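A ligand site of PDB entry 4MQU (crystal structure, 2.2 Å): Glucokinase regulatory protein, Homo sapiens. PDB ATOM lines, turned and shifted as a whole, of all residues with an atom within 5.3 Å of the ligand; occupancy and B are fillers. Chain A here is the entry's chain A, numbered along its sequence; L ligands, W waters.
A nitrogen (N1) of the ligand lies within hydrogen-bond range of the backbone carbonyl oxygen (O) of Gly 192, 2.7 Å away. N1 of the ligand lies within hydrogen-bond range of O of Met 224 (2.8 Å). NE of Arg 536 sits at hydrogen-bond distance from O3 of the ligand (3.1 Å).
The side-chain carboxylate (OE1) of Glu 43 is in salt-bridge range of the guanidinium group (NE) of Arg 529 (2.7 Å). The side-chain carboxylate (OE2) of Glu 36 is in salt-bridge range of the guanidinium group (NH2) of Arg 536. A ring nitrogen (ND1) of His 515 sits at hydrogen-bond distance from the side-chain hydroxyl (OG) of Ser 266. The side-chain carboxylate (OD2) of Asp 228 is in hydrogen-bond range of the indole nitrogen (NE1) of Trp 528 (3.0 Å). The side-chain carboxylate (OD1) of Asp 228 lies within salt-bridge range of the guanidinium group (NE) of Arg 226 (2.8 Å). N of Arg 226 is in hydrogen-bond range of O of Leu 193, 3.0 Å away. The side-chain amide nitrogen (ND2) of Asn 220 is in hydrogen-bond range of the side-chain hydroxyl (OG1) of Thr 42, at 3.1 Å. The backbone NH (N) of Tyr 35 lies close to the backbone carbonyl oxygen (O) of Trp 30, at 3.3 Å.
The backbone carbonyl oxygen (O) of Glu 43 lies close to a fluorine (F4) of the ligand (2.9 Å). An oxygen (O2) of the ligand lies close to the side-chain carboxylate (OD1) of Asp 228 (3.4 Å). NE2 of His 515 lies close to F1 of the ligand, at 3.4 Å. F2 of the ligand sits close to O of Ala 532, 2.8 Å away. The backbone NH of Met 533 sits close to a fluorine (F2) of the ligand. Tyr 35 touches the ligand (OH to C15, 3.9 Å). CG1 of Val 39 touches F5 of the ligand, 3.4 Å away. Pro 40 touches the ligand. Ser 45 touches the ligand (N to F4, 3.7 Å). CB of Ser 194 touches C2 of the ligand (3.8 Å). ND2 of Asn 220 touches N1 of the ligand, at 3.5 Å. Ala 225 touches the ligand. Arg 226 touches the ligand (CA to N2, 3.5 Å). Lys 525 touches the ligand. Trp 528 touches the ligand (O to C10, 3.4 Å). Arg 529 touches the ligand (CA to C12, 3.8 Å). Hydrophobic or aromatic side chains within 4 Å of the ligand: Val 39, Pro 40, His 515, Trp 528, Ala 532 and Met 533. The nearest printed residue that does not touch the ligand is Lys 44 (4.01 Å).
Water W1 lies within hydrogen-bond range of O3 of the ligand (2.5 Å), O of Ala 532 (2.6 Å) and OH of Tyr 35 (2.8 Å).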
ATOM      1  N   HIS A  20      15.671  28.988  21.662  1.00  0.00           N
ATOM      2  CA  HIS A  20      14.264  28.790  21.366  1.00  0.00           C
ATOM      3  C   HIS A  20      13.990  27.602  20.401  1.00  0.00           C
ATOM      4  O   HIS A  20      12.855  27.136  20.274  1.00  0.00           O
ATOM      5  CB  HIS A  20      13.730  30.100  20.777  1.00  0.00           C
ATOM      6  CG  HIS A  20      14.170  30.367  19.382  1.00  0.00           C
ATOM      7  ND1 HIS A  20      15.374  30.963  19.082  1.00  0.00           N
ATOM      8  CD2 HIS A  20      13.594  30.067  18.192  1.00  0.00           C
ATOM      9  CE1 HIS A  20      15.513  31.038  17.769  1.00  0.00           C
ATOM     10  NE2 HIS A  20      14.445  30.500  17.210  1.00  0.00           N
ATOM     11  N   VAL A  21      15.045  27.131  19.718  1.00  0.00           N
ATOM     12  CA  VAL A  21      14.904  26.144  18.691  1.00  0.00           C
ATOM     13  C   VAL A  21      14.568  24.840  19.374  1.00  0.00           C
ATOM     14  O   VAL A  21      15.255  24.471  20.264  1.00  0.00           O
ATOM     15  CB  VAL A  21      16.211  26.071  17.848  1.00  0.00           C
ATOM     16  CG1 VAL A  21      16.215  24.917  16.887  1.00  0.00           C
ATOM     17  CG2 VAL A  21      16.375  27.315  17.023  1.00  0.00           C
ATOM     18  N   TRP A  30       8.463  12.249  16.427  1.00  0.00           N
ATOM     19  CA  TRP A  30       8.213  13.629  15.952  1.00  0.00           C
ATOM     20  C   TRP A  30       6.863  14.205  16.373  1.00  0.00           C
ATOM     21  O   TRP A  30       6.767  15.397  16.693  1.00  0.00           O
ATOM     22  CB  TRP A  30       8.349  13.697  14.453  1.00  0.00           C
ATOM     23  CG  TRP A  30       9.773  13.641  13.975  1.00  0.00           C
ATOM     24  CD1 TRP A  30      10.528  12.522  13.739  1.00  0.00           C
ATOM     25  CD2 TRP A  30      10.608  14.769  13.643  1.00  0.00           C
ATOM     26  NE1 TRP A  30      11.794  12.882  13.301  1.00  0.00           N
ATOM     27  CE2 TRP A  30      11.862  14.253  13.233  1.00  0.00           C
ATOM     28  CE3 TRP A  30      10.420  16.157  13.657  1.00  0.00           C
ATOM     29  CZ2 TRP A  30      12.898  15.079  12.840  1.00  0.00           C
ATOM     30  CZ3 TRP A  30      11.455  16.974  13.279  1.00  0.00           C
ATOM     31  CH2 TRP A  30      12.680  16.433  12.864  1.00  0.00           C
ATOM     32  N   TYR A  35       6.701  17.951  18.847  1.00  0.00           N
ATOM     33  CA  TYR A  35       7.486  18.809  17.960  1.00  0.00           C
ATOM     34  C   TYR A  35       6.556  19.345  16.891  1.00  0.00           C
ATOM     35  O   TYR A  35       6.466  20.566  16.697  1.00  0.00           O
ATOM     36  CB  TYR A  35       8.644  18.052  17.289  1.00  0.00           C
ATOM     37  CG  TYR A  35       9.486  18.905  16.372  1.00  0.00           C
ATOM     38  CD1 TYR A  35       9.041  19.255  15.094  1.00  0.00           C
ATOM     39  CD2 TYR A  35      10.700  19.374  16.772  1.00  0.00           C
ATOM     40  CE1 TYR A  35       9.804  20.047  14.260  1.00  0.00           C
ATOM     41  CE2 TYR A  35      11.467  20.157  15.940  1.00  0.00           C
ATOM     42  CZ  TYR A  35      11.007  20.471  14.679  1.00  0.00           C
ATOM     43  OH  TYR A  35      11.790  21.257  13.884  1.00  0.00           O
ATOM     44  N   GLU A  36       5.874  18.416  16.207  1.00  0.00           N
ATOM     45  CA  GLU A  36       4.971  18.772  15.116  1.00  0.00           C
ATOM     46  C   GLU A  36       3.856  19.666  15.556  1.00  0.00           C
ATOM     47  O   GLU A  36       3.404  20.484  14.781  1.00  0.00           O
ATOM     48  CB  GLU A  36       4.370  17.538  14.458  1.00  0.00           C
ATOM     49  CG  GLU A  36       4.694  17.481  12.973  1.00  0.00           C
ATOM     50  CD  GLU A  36       5.732  16.441  12.634  1.00  0.00           C
ATOM     51  OE1 GLU A  36       5.391  15.242  12.611  1.00  0.00           O
ATOM     52  OE2 GLU A  36       6.866  16.820  12.346  1.00  0.00           O
ATOM     53  N   VAL A  39       5.017  23.194  15.023  1.00  0.00           N
ATOM     54  CA  VAL A  39       5.363  23.794  13.720  1.00  0.00           C
ATOM     55  C   VAL A  39       4.228  24.667  13.304  1.00  0.00           C
ATOM     56  O   VAL A  39       3.075  24.187  13.200  1.00  0.00           O
ATOM     57  CB  VAL A  39       5.715  22.765  12.629  1.00  0.00           C
ATOM     58  CG1 VAL A  39       6.066  23.464  11.311  1.00  0.00           C
ATOM     59  CG2 VAL A  39       6.903  21.890  13.084  1.00  0.00           C
ATOM     60  N   PRO A  40       4.519  25.960  13.087  1.00  0.00           N
ATOM     61  CA  PRO A  40       3.380  26.809  12.670  1.00  0.00           C
ATOM     62  C   PRO A  40       2.694  26.263  11.437  1.00  0.00           C
ATOM     63  O   PRO A  40       3.315  25.616  10.609  1.00  0.00           O
ATOM     64  CB  PRO A  40       4.017  28.164  12.402  1.00  0.00           C
ATOM     65  CG  PRO A  40       5.289  28.165  13.206  1.00  0.00           C
ATOM     66  CD  PRO A  40       5.753  26.735  13.259  1.00  0.00           C
ATOM     67  N   THR A  42       1.755  27.494   8.818  1.00  0.00           N
ATOM     68  CA  THR A  42       2.282  28.033   7.586  1.00  0.00           C
ATOM     69  C   THR A  42       3.598  27.414   7.135  1.00  0.00           C
ATOM     70  O   THR A  42       4.010  27.586   5.984  1.00  0.00           O
ATOM     71  CB  THR A  42       2.439  29.573   7.661  1.00  0.00           C
ATOM     72  OG1 THR A  42       3.351  29.959   8.718  1.00  0.00           O
ATOM     73  CG2 THR A  42       1.081  30.216   7.939  1.00  0.00           C
ATOM     74  N   GLU A  43       4.280  26.725   8.053  1.00  0.00           N
ATOM     75  CA  GLU A  43       5.542  26.084   7.718  1.00  0.00           C
ATOM     76  C   GLU A  43       5.410  24.613   7.598  1.00  0.00           C
ATOM     77  O   GLU A  43       6.356  23.958   7.219  1.00  0.00           O
ATOM     78  CB  GLU A  43       6.588  26.398   8.788  1.00  0.00           C
ATOM     79  CG  GLU A  43       6.810  27.894   8.946  1.00  0.00           C
ATOM     80  CD  GLU A  43       7.777  28.469   7.919  1.00  0.00           C
ATOM     81  OE1 GLU A  43       8.618  27.714   7.389  1.00  0.00           O
ATOM     82  OE2 GLU A  43       7.701  29.678   7.646  1.00  0.00           O
ATOM     83  N   LYS A  44       4.227  24.080   7.891  1.00  0.00           N
ATOM     84  CA  LYS A  44       4.049  22.649   7.851  1.00  0.00           C
ATOM     85  C   LYS A  44       4.189  22.050   6.444  1.00  0.00           C
ATOM     86  O   LYS A  44       4.056  22.731   5.409  1.00  0.00           O
ATOM     87  CB  LYS A  44       2.710  22.244   8.497  1.00  0.00           C
ATOM     88  CG  LYS A  44       2.646  22.307  10.048  1.00  0.00           C
ATOM     89  CD  LYS A  44       1.389  21.570  10.529  1.00  0.00           C
ATOM     90  CE  LYS A  44       0.751  22.064  11.830  1.00  0.00           C
ATOM     91  NZ  LYS A  44       1.688  21.924  12.978  1.00  0.00           N
ATOM     92  N   SER A  45       4.583  20.781   6.463  1.00  0.00           N
ATOM     93  CA  SER A  45       4.529  19.898   5.325  1.00  0.00           C
ATOM     94  C   SER A  45       3.069  19.509   5.025  1.00  0.00           C
ATOM     95  O   SER A  45       2.426  18.868   5.854  1.00  0.00           O
ATOM     96  CB  SER A  45       5.311  18.606   5.643  1.00  0.00           C
ATOM     97  OG  SER A  45       5.142  17.674   4.618  1.00  0.00           O
ATOM     98  N   GLY A 192       2.565  34.314   8.074  1.00  0.00           N
ATOM     99  CA  GLY A 192       3.117  33.474   9.123  1.00  0.00           C
ATOM    100  C   GLY A 192       3.039  34.136  10.486  1.00  0.00           C
ATOM    101  O   GLY A 192       3.528  33.568  11.426  1.00  0.00           O
ATOM    102  N   LEU A 193       2.374  35.277  10.584  1.00  0.00           N
ATOM    103  CA  LEU A 193       2.427  36.146  11.760  1.00  0.00           C
ATOM    104  C   LEU A 193       3.930  36.248  12.193  1.00  0.00           C
ATOM    105  O   LEU A 193       4.301  35.919  13.300  1.00  0.00           O
ATOM    106  CB  LEU A 193       1.557  35.598  12.867  1.00  0.00           C
ATOM    107  CG  LEU A 193       0.039  35.556  12.597  1.00  0.00           C
ATOM    108  CD1 LEU A 193      -0.673  35.184  13.899  1.00  0.00           C
ATOM    109  CD2 LEU A 193      -0.504  36.881  12.096  1.00  0.00           C
ATOM    110  N   SER A 194       4.750  36.713  11.266  1.00  0.00           N
ATOM    111  CA  SER A 194       6.157  36.529  11.332  1.00  0.00           C
ATOM    112  C   SER A 194       7.012  37.779  11.005  1.00  0.00           C
ATOM    113  O   SER A 194       8.071  37.916  11.576  1.00  0.00           O
ATOM    114  CB  SER A 194       6.517  35.439  10.361  1.00  0.00           C
ATOM    115  OG  SER A 194       7.878  35.538   9.961  1.00  0.00           O
ATOM    116  N   ASN A 220      -1.896  31.838  11.019  1.00  0.00           N
ATOM    117  CA  ASN A 220      -1.624  30.981  12.148  1.00  0.00           C
ATOM    118  C   ASN A 220      -2.460  31.391  13.358  1.00  0.00           C
ATOM    119  O   ASN A 220      -2.775  32.550  13.552  1.00  0.00           O
ATOM    120  CB  ASN A 220      -0.135  31.109  12.520  1.00  0.00           C
ATOM    121  CG  ASN A 220       0.766  30.340  11.584  1.00  0.00           C
ATOM    122  OD1 ASN A 220       0.498  29.181  11.276  1.00  0.00           O
ATOM    123  ND2 ASN A 220       1.854  30.964  11.179  1.00  0.00           N
ATOM    124  N   MET A 224       0.893  30.286  17.596  1.00  0.00           N
ATOM    125  CA  MET A 224       1.969  29.841  16.729  1.00  0.00           C
ATOM    126  C   MET A 224       2.610  31.034  16.050  1.00  0.00           C
ATOM    127  O   MET A 224       3.333  30.909  15.056  1.00  0.00           O
ATOM    128  CB  MET A 224       1.408  28.925  15.643  1.00  0.00           C
ATOM    129  CG  MET A 224       1.186  27.479  16.046  1.00  0.00           C
ATOM    130  SD  MET A 224       0.048  26.695  14.830  1.00  0.00           S
ATOM    131  CE  MET A 224       0.376  24.971  15.146  1.00  0.00           C
ATOM    132  N   ALA A 225       2.304  32.218  16.556  1.00  0.00           N
ATOM    133  CA  ALA A 225       2.871  33.441  16.014  1.00  0.00           C
ATOM    134  C   ALA A 225       4.335  33.416  16.293  1.00  0.00           C
ATOM    135  O   ALA A 225       4.775  32.834  17.266  1.00  0.00           O
ATOM    136  CB  ALA A 225       2.237  34.620  16.656  1.00  0.00           C
ATOM    137  N   ARG A 226       5.121  34.048  15.441  1.00  0.00           N
ATOM    138  CA  ARG A 226       6.585  33.959  15.575  1.00  0.00           C
ATOM    139  C   ARG A 226       7.037  34.513  16.908  1.00  0.00           C
ATOM    140  O   ARG A 226       6.499  35.515  17.402  1.00  0.00           O
ATOM    141  CB  ARG A 226       7.270  34.697  14.431  1.00  0.00           C
ATOM    142  CG  ARG A 226       8.675  34.270  14.238  1.00  0.00           C
ATOM    143  CD  ARG A 226       9.234  34.859  12.966  1.00  0.00           C
ATOM    144  NE  ARG A 226      10.681  34.853  12.998  1.00  0.00           N
ATOM    145  CZ  ARG A 226      11.462  35.375  12.054  1.00  0.00           C
ATOM    146  NH1 ARG A 226      10.929  35.924  10.957  1.00  0.00           N
ATOM    147  NH2 ARG A 226      12.774  35.365  12.190  1.00  0.00           N
ATOM    148  N   ASN A 227       8.005  33.819  17.517  1.00  0.00           N
ATOM    149  CA  ASN A 227       8.423  34.162  18.870  1.00  0.00           C
ATOM    150  C   ASN A 227       9.881  34.237  19.160  1.00  0.00           C
ATOM    151  O   ASN A 227      10.202  34.391  20.289  1.00  0.00           O
ATOM    152  CB  ASN A 227       7.796  33.251  19.912  1.00  0.00           C
ATOM    153  CG  ASN A 227       7.676  33.919  21.287  1.00  0.00           C
ATOM    154  OD1 ASN A 227       7.327  35.094  21.421  1.00  0.00           O
ATOM    155  ND2 ASN A 227       7.986  33.186  22.291  1.00  0.00           N
ATOM    156  N   ASP A 228      10.756  34.178  18.168  1.00  0.00           N
ATOM    157  CA  ASP A 228      12.174  34.462  18.374  1.00  0.00           C
ATOM    158  C   ASP A 228      12.426  35.995  18.375  1.00  0.00           C
ATOM    159  O   ASP A 228      11.620  36.726  17.820  1.00  0.00           O
ATOM    160  CB  ASP A 228      13.058  33.751  17.323  1.00  0.00           C
ATOM    161  CG  ASP A 228      12.693  34.124  15.886  1.00  0.00           C
ATOM    162  OD1 ASP A 228      11.563  33.767  15.474  1.00  0.00           O
ATOM    163  OD2 ASP A 228      13.521  34.707  15.138  1.00  0.00           O
ATOM    164  N   SER A 266       5.924  23.552   1.130  1.00  0.00           N
ATOM    165  CA  SER A 266       6.112  23.901   2.514  1.00  0.00           C
ATOM    166  C   SER A 266       6.679  25.305   2.677  1.00  0.00           C
ATOM    167  O   SER A 266       7.750  25.613   2.179  1.00  0.00           O
ATOM    168  CB  SER A 266       7.017  22.877   3.219  1.00  0.00           C
ATOM    169  OG  SER A 266       6.514  21.551   3.029  1.00  0.00           O
ATOM    170  N   HIS A 515       9.442  20.076  -0.098  1.00  0.00           N
ATOM    171  CA  HIS A 515      10.323  21.080   0.525  1.00  0.00           C
ATOM    172  C   HIS A 515      11.315  21.602  -0.536  1.00  0.00           C
ATOM    173  O   HIS A 515      11.802  20.828  -1.374  1.00  0.00           O
ATOM    174  CB  HIS A 515      11.151  20.448   1.674  1.00  0.00           C
ATOM    175  CG  HIS A 515      10.337  20.019   2.864  1.00  0.00           C
ATOM    176  ND1 HIS A 515       9.581  20.911   3.605  1.00  0.00           N
ATOM    177  CD2 HIS A 515      10.179  18.807   3.452  1.00  0.00           C
ATOM    178  CE1 HIS A 515       8.993  20.261   4.597  1.00  0.00           C
ATOM    179  NE2 HIS A 515       9.347  18.991   4.529  1.00  0.00           N
ATOM    180  N   SER A 524      15.952  36.105   8.140  1.00  0.00           N
ATOM    181  CA  SER A 524      16.016  35.265   9.356  1.00  0.00           C
ATOM    182  C   SER A 524      15.081  34.060   9.315  1.00  0.00           C
ATOM    183  O   SER A 524      15.468  32.906   9.629  1.00  0.00           O
ATOM    184  CB  SER A 524      15.699  36.126  10.573  1.00  0.00           C
ATOM    185  OG  SER A 524      14.450  36.808  10.442  1.00  0.00           O
ATOM    186  N   LYS A 525      13.840  34.311   8.912  1.00  0.00           N
ATOM    187  CA  LYS A 525      12.899  33.189   8.697  1.00  0.00           C
ATOM    188  C   LYS A 525      13.429  32.059   7.817  1.00  0.00           C
ATOM    189  O   LYS A 525      13.249  30.873   8.102  1.00  0.00           O
ATOM    190  CB  LYS A 525      11.585  33.721   8.141  1.00  0.00           C
ATOM    191  CG  LYS A 525      10.549  32.669   7.823  1.00  0.00           C
ATOM    192  CD  LYS A 525       9.228  33.345   7.384  1.00  0.00           C
ATOM    193  CE  LYS A 525       9.285  33.995   6.017  1.00  0.00           C
ATOM    194  NZ  LYS A 525       7.977  34.655   5.792  1.00  0.00           N
ATOM    195  N   TRP A 528      15.936  30.191   9.694  1.00  0.00           N
ATOM    196  CA  TRP A 528      15.305  29.198  10.566  1.00  0.00           C
ATOM    197  C   TRP A 528      14.760  28.007   9.784  1.00  0.00           C
ATOM    198  O   TRP A 528      14.917  26.864  10.207  1.00  0.00           O
ATOM    199  CB  TRP A 528      14.237  29.830  11.463  1.00  0.00           C
ATOM    200  CG  TRP A 528      14.808  30.840  12.391  1.00  0.00           C
ATOM    201  CD1 TRP A 528      14.432  32.132  12.502  1.00  0.00           C
ATOM    202  CD2 TRP A 528      15.863  30.653  13.336  1.00  0.00           C
ATOM    203  NE1 TRP A 528      15.155  32.763  13.480  1.00  0.00           N
ATOM    204  CE2 TRP A 528      16.056  31.877  14.003  1.00  0.00           C
ATOM    205  CE3 TRP A 528      16.642  29.550  13.710  1.00  0.00           C
ATOM    206  CZ2 TRP A 528      17.024  32.053  15.004  1.00  0.00           C
ATOM    207  CZ3 TRP A 528      17.603  29.718  14.739  1.00  0.00           C
ATOM    208  CH2 TRP A 528      17.785  30.970  15.355  1.00  0.00           C
ATOM    209  N   ARG A 529      14.149  28.286   8.621  1.00  0.00           N
ATOM    210  CA  ARG A 529      13.605  27.218   7.783  1.00  0.00           C
ATOM    211  C   ARG A 529      14.728  26.273   7.348  1.00  0.00           C
ATOM    212  O   ARG A 529      14.554  25.060   7.328  1.00  0.00           O
ATOM    213  CB  ARG A 529      12.879  27.776   6.548  1.00  0.00           C
ATOM    214  CG  ARG A 529      12.117  26.687   5.748  1.00  0.00           C
ATOM    215  CD  ARG A 529      11.205  27.291   4.694  1.00  0.00           C
ATOM    216  NE  ARG A 529      10.233  28.281   5.240  1.00  0.00           N
ATOM    217  CZ  ARG A 529       9.812  29.377   4.612  1.00  0.00           C
ATOM    218  NH1 ARG A 529      10.282  29.687   3.414  1.00  0.00           N
ATOM    219  NH2 ARG A 529       8.938  30.201   5.173  1.00  0.00           N
ATOM    220  N   LEU A 531      17.604  25.625   8.974  1.00  0.00           N
ATOM    221  CA  LEU A 531      17.993  24.830  10.153  1.00  0.00           C
ATOM    222  C   LEU A 531      16.973  23.706  10.413  1.00  0.00           C
ATOM    223  O   LEU A 531      17.336  22.578  10.692  1.00  0.00           O
ATOM    224  CB  LEU A 531      18.102  25.745  11.383  1.00  0.00           C
ATOM    225  CG  LEU A 531      18.353  25.035  12.723  1.00  0.00           C
ATOM    226  CD1 LEU A 531      19.561  24.132  12.578  1.00  0.00           C
ATOM    227  CD2 LEU A 531      18.504  26.066  13.831  1.00  0.00           C
ATOM    228  N   ALA A 532      15.698  24.027  10.309  1.00  0.00           N
ATOM    229  CA  ALA A 532      14.638  23.027  10.449  1.00  0.00           C
ATOM    230  C   ALA A 532      14.762  21.905   9.447  1.00  0.00           C
ATOM    231  O   ALA A 532      14.500  20.735   9.766  1.00  0.00           O
ATOM    232  CB  ALA A 532      13.286  23.705  10.244  1.00  0.00           C
ATOM    233  N   MET A 533      15.070  22.244   8.194  1.00  0.00           N
ATOM    234  CA  MET A 533      15.200  21.222   7.177  1.00  0.00           C
ATOM    235  C   MET A 533      16.424  20.349   7.462  1.00  0.00           C
ATOM    236  O   MET A 533      16.374  19.128   7.303  1.00  0.00           O
ATOM    237  CB  MET A 533      15.233  21.838   5.807  1.00  0.00           C
ATOM    238  CG  MET A 533      13.845  22.301   5.390  1.00  0.00           C
ATOM    239  SD  MET A 533      13.835  22.857   3.710  1.00  0.00           S
ATOM    240  CE  MET A 533      14.984  24.211   3.648  1.00  0.00           C
ATOM    241  N   GLN A 535      17.548  19.600  10.459  1.00  0.00           N
ATOM    242  CA  GLN A 535      17.110  18.650  11.507  1.00  0.00           C
ATOM    243  C   GLN A 535      16.238  17.542  10.952  1.00  0.00           C
ATOM    244  O   GLN A 535      16.439  16.376  11.278  1.00  0.00           O
ATOM    245  CB  GLN A 535      16.322  19.348  12.608  1.00  0.00           C
ATOM    246  CG  GLN A 535      17.134  20.413  13.300  1.00  0.00           C
ATOM    247  CD  GLN A 535      16.321  21.211  14.296  1.00  0.00           C
ATOM    248  OE1 GLN A 535      15.866  22.316  13.999  1.00  0.00           O
ATOM    249  NE2 GLN A 535      16.104  20.620  15.485  1.00  0.00           N
ATOM    250  N   ARG A 536      15.258  17.922  10.135  1.00  0.00           N
ATOM    251  CA  ARG A 536      14.249  17.028   9.617  1.00  0.00           C
ATOM    252  C   ARG A 536      14.873  15.928   8.738  1.00  0.00           C
ATOM    253  O   ARG A 536      14.649  14.769   8.973  1.00  0.00           O
ATOM    254  CB  ARG A 536      13.181  17.821   8.838  1.00  0.00           C
ATOM    255  CG  ARG A 536      12.104  16.976   8.159  1.00  0.00           C
ATOM    256  CD  ARG A 536      11.149  16.316   9.123  1.00  0.00           C
ATOM    257  NE  ARG A 536      10.200  17.312   9.648  1.00  0.00           N
ATOM    258  CZ  ARG A 536       9.122  17.039  10.381  1.00  0.00           C
ATOM    259  NH1 ARG A 536       8.828  15.787  10.696  1.00  0.00           N
ATOM    260  NH2 ARG A 536       8.331  18.023  10.790  1.00  0.00           N
HETATM  261  C1  LIG L   1       8.166  31.601  11.406  1.00  0.00           C
HETATM  262  C2  LIG L   1       6.790  31.794  11.539  1.00  0.00           C
HETATM  263  C3  LIG L   1       6.167  31.496  12.740  1.00  0.00           C
HETATM  264  N1  LIG L   1       4.882  31.683  12.866  1.00  0.00           N
HETATM  265  N2  LIG L   1       6.877  31.015  13.797  1.00  0.00           N
HETATM  266  C4  LIG L   1       8.204  30.820  13.704  1.00  0.00           C
HETATM  267  C5  LIG L   1       8.885  31.109  12.498  1.00  0.00           C
HETATM  268  S1  LIG L   1      10.562  30.780  12.366  1.00  0.00           S
HETATM  269  O1  LIG L   1      11.176  31.652  11.320  1.00  0.00           O
HETATM  270  O2  LIG L   1      11.183  30.942  13.703  1.00  0.00           O
HETATM  271  N3  LIG L   1      10.760  29.232  11.983  1.00  0.00           N
HETATM  272  C6  LIG L   1       9.887  28.379  12.809  1.00  0.00           C
HETATM  273  C7  LIG L   1      10.161  26.857  12.558  1.00  0.00           C
HETATM  274  C8  LIG L   1      11.575  26.577  12.890  1.00  0.00           C
HETATM  275  C9  LIG L   1      12.719  26.361  13.134  1.00  0.00           C
HETATM  276  C10 LIG L   1      14.129  26.092  13.418  1.00  0.00           C
HETATM  277  C11 LIG L   1      10.431  29.060  10.573  1.00  0.00           C
HETATM  278  C12 LIG L   1      10.638  27.607  10.152  1.00  0.00           C
HETATM  279  N4  LIG L   1      10.139  26.585  11.090  1.00  0.00           N
HETATM  280  C13 LIG L   1      10.047  25.317  10.582  1.00  0.00           C
HETATM  281  C14 LIG L   1      10.069  24.225  11.423  1.00  0.00           C
HETATM  282  C15 LIG L   1       9.983  22.944  10.896  1.00  0.00           C
HETATM  283  C16 LIG L   1       9.971  25.077   9.222  1.00  0.00           C
HETATM  284  C17 LIG L   1       9.859  23.787   8.706  1.00  0.00           C
HETATM  285  C18 LIG L   1       9.890  22.698   9.543  1.00  0.00           C
HETATM  286  C19 LIG L   1       9.829  21.251   9.022  1.00  0.00           C
HETATM  287  C20 LIG L   1      10.881  21.049   7.932  1.00  0.00           C
HETATM  288  F1  LIG L   1      10.885  19.786   7.513  1.00  0.00           F
HETATM  289  F2  LIG L   1      12.116  21.342   8.399  1.00  0.00           F
HETATM  290  F3  LIG L   1      10.595  21.869   6.922  1.00  0.00           F
HETATM  291  C21 LIG L   1       8.431  20.853   8.549  1.00  0.00           C
HETATM  292  F4  LIG L   1       8.024  21.606   7.525  1.00  0.00           F
HETATM  293  F5  LIG L   1       7.575  20.933   9.549  1.00  0.00           F
HETATM  294  F6  LIG L   1       8.438  19.593   8.138  1.00  0.00           F
HETATM  295  O3  LIG L   1      10.238  20.415  10.063  1.00  0.00           O
HETATM  296  O   HOH W   1      12.414  20.312  11.299  1.00  0.00           O
HETATM  297  O   HOH W   2       6.590  29.645  16.081  1.00  0.00           O
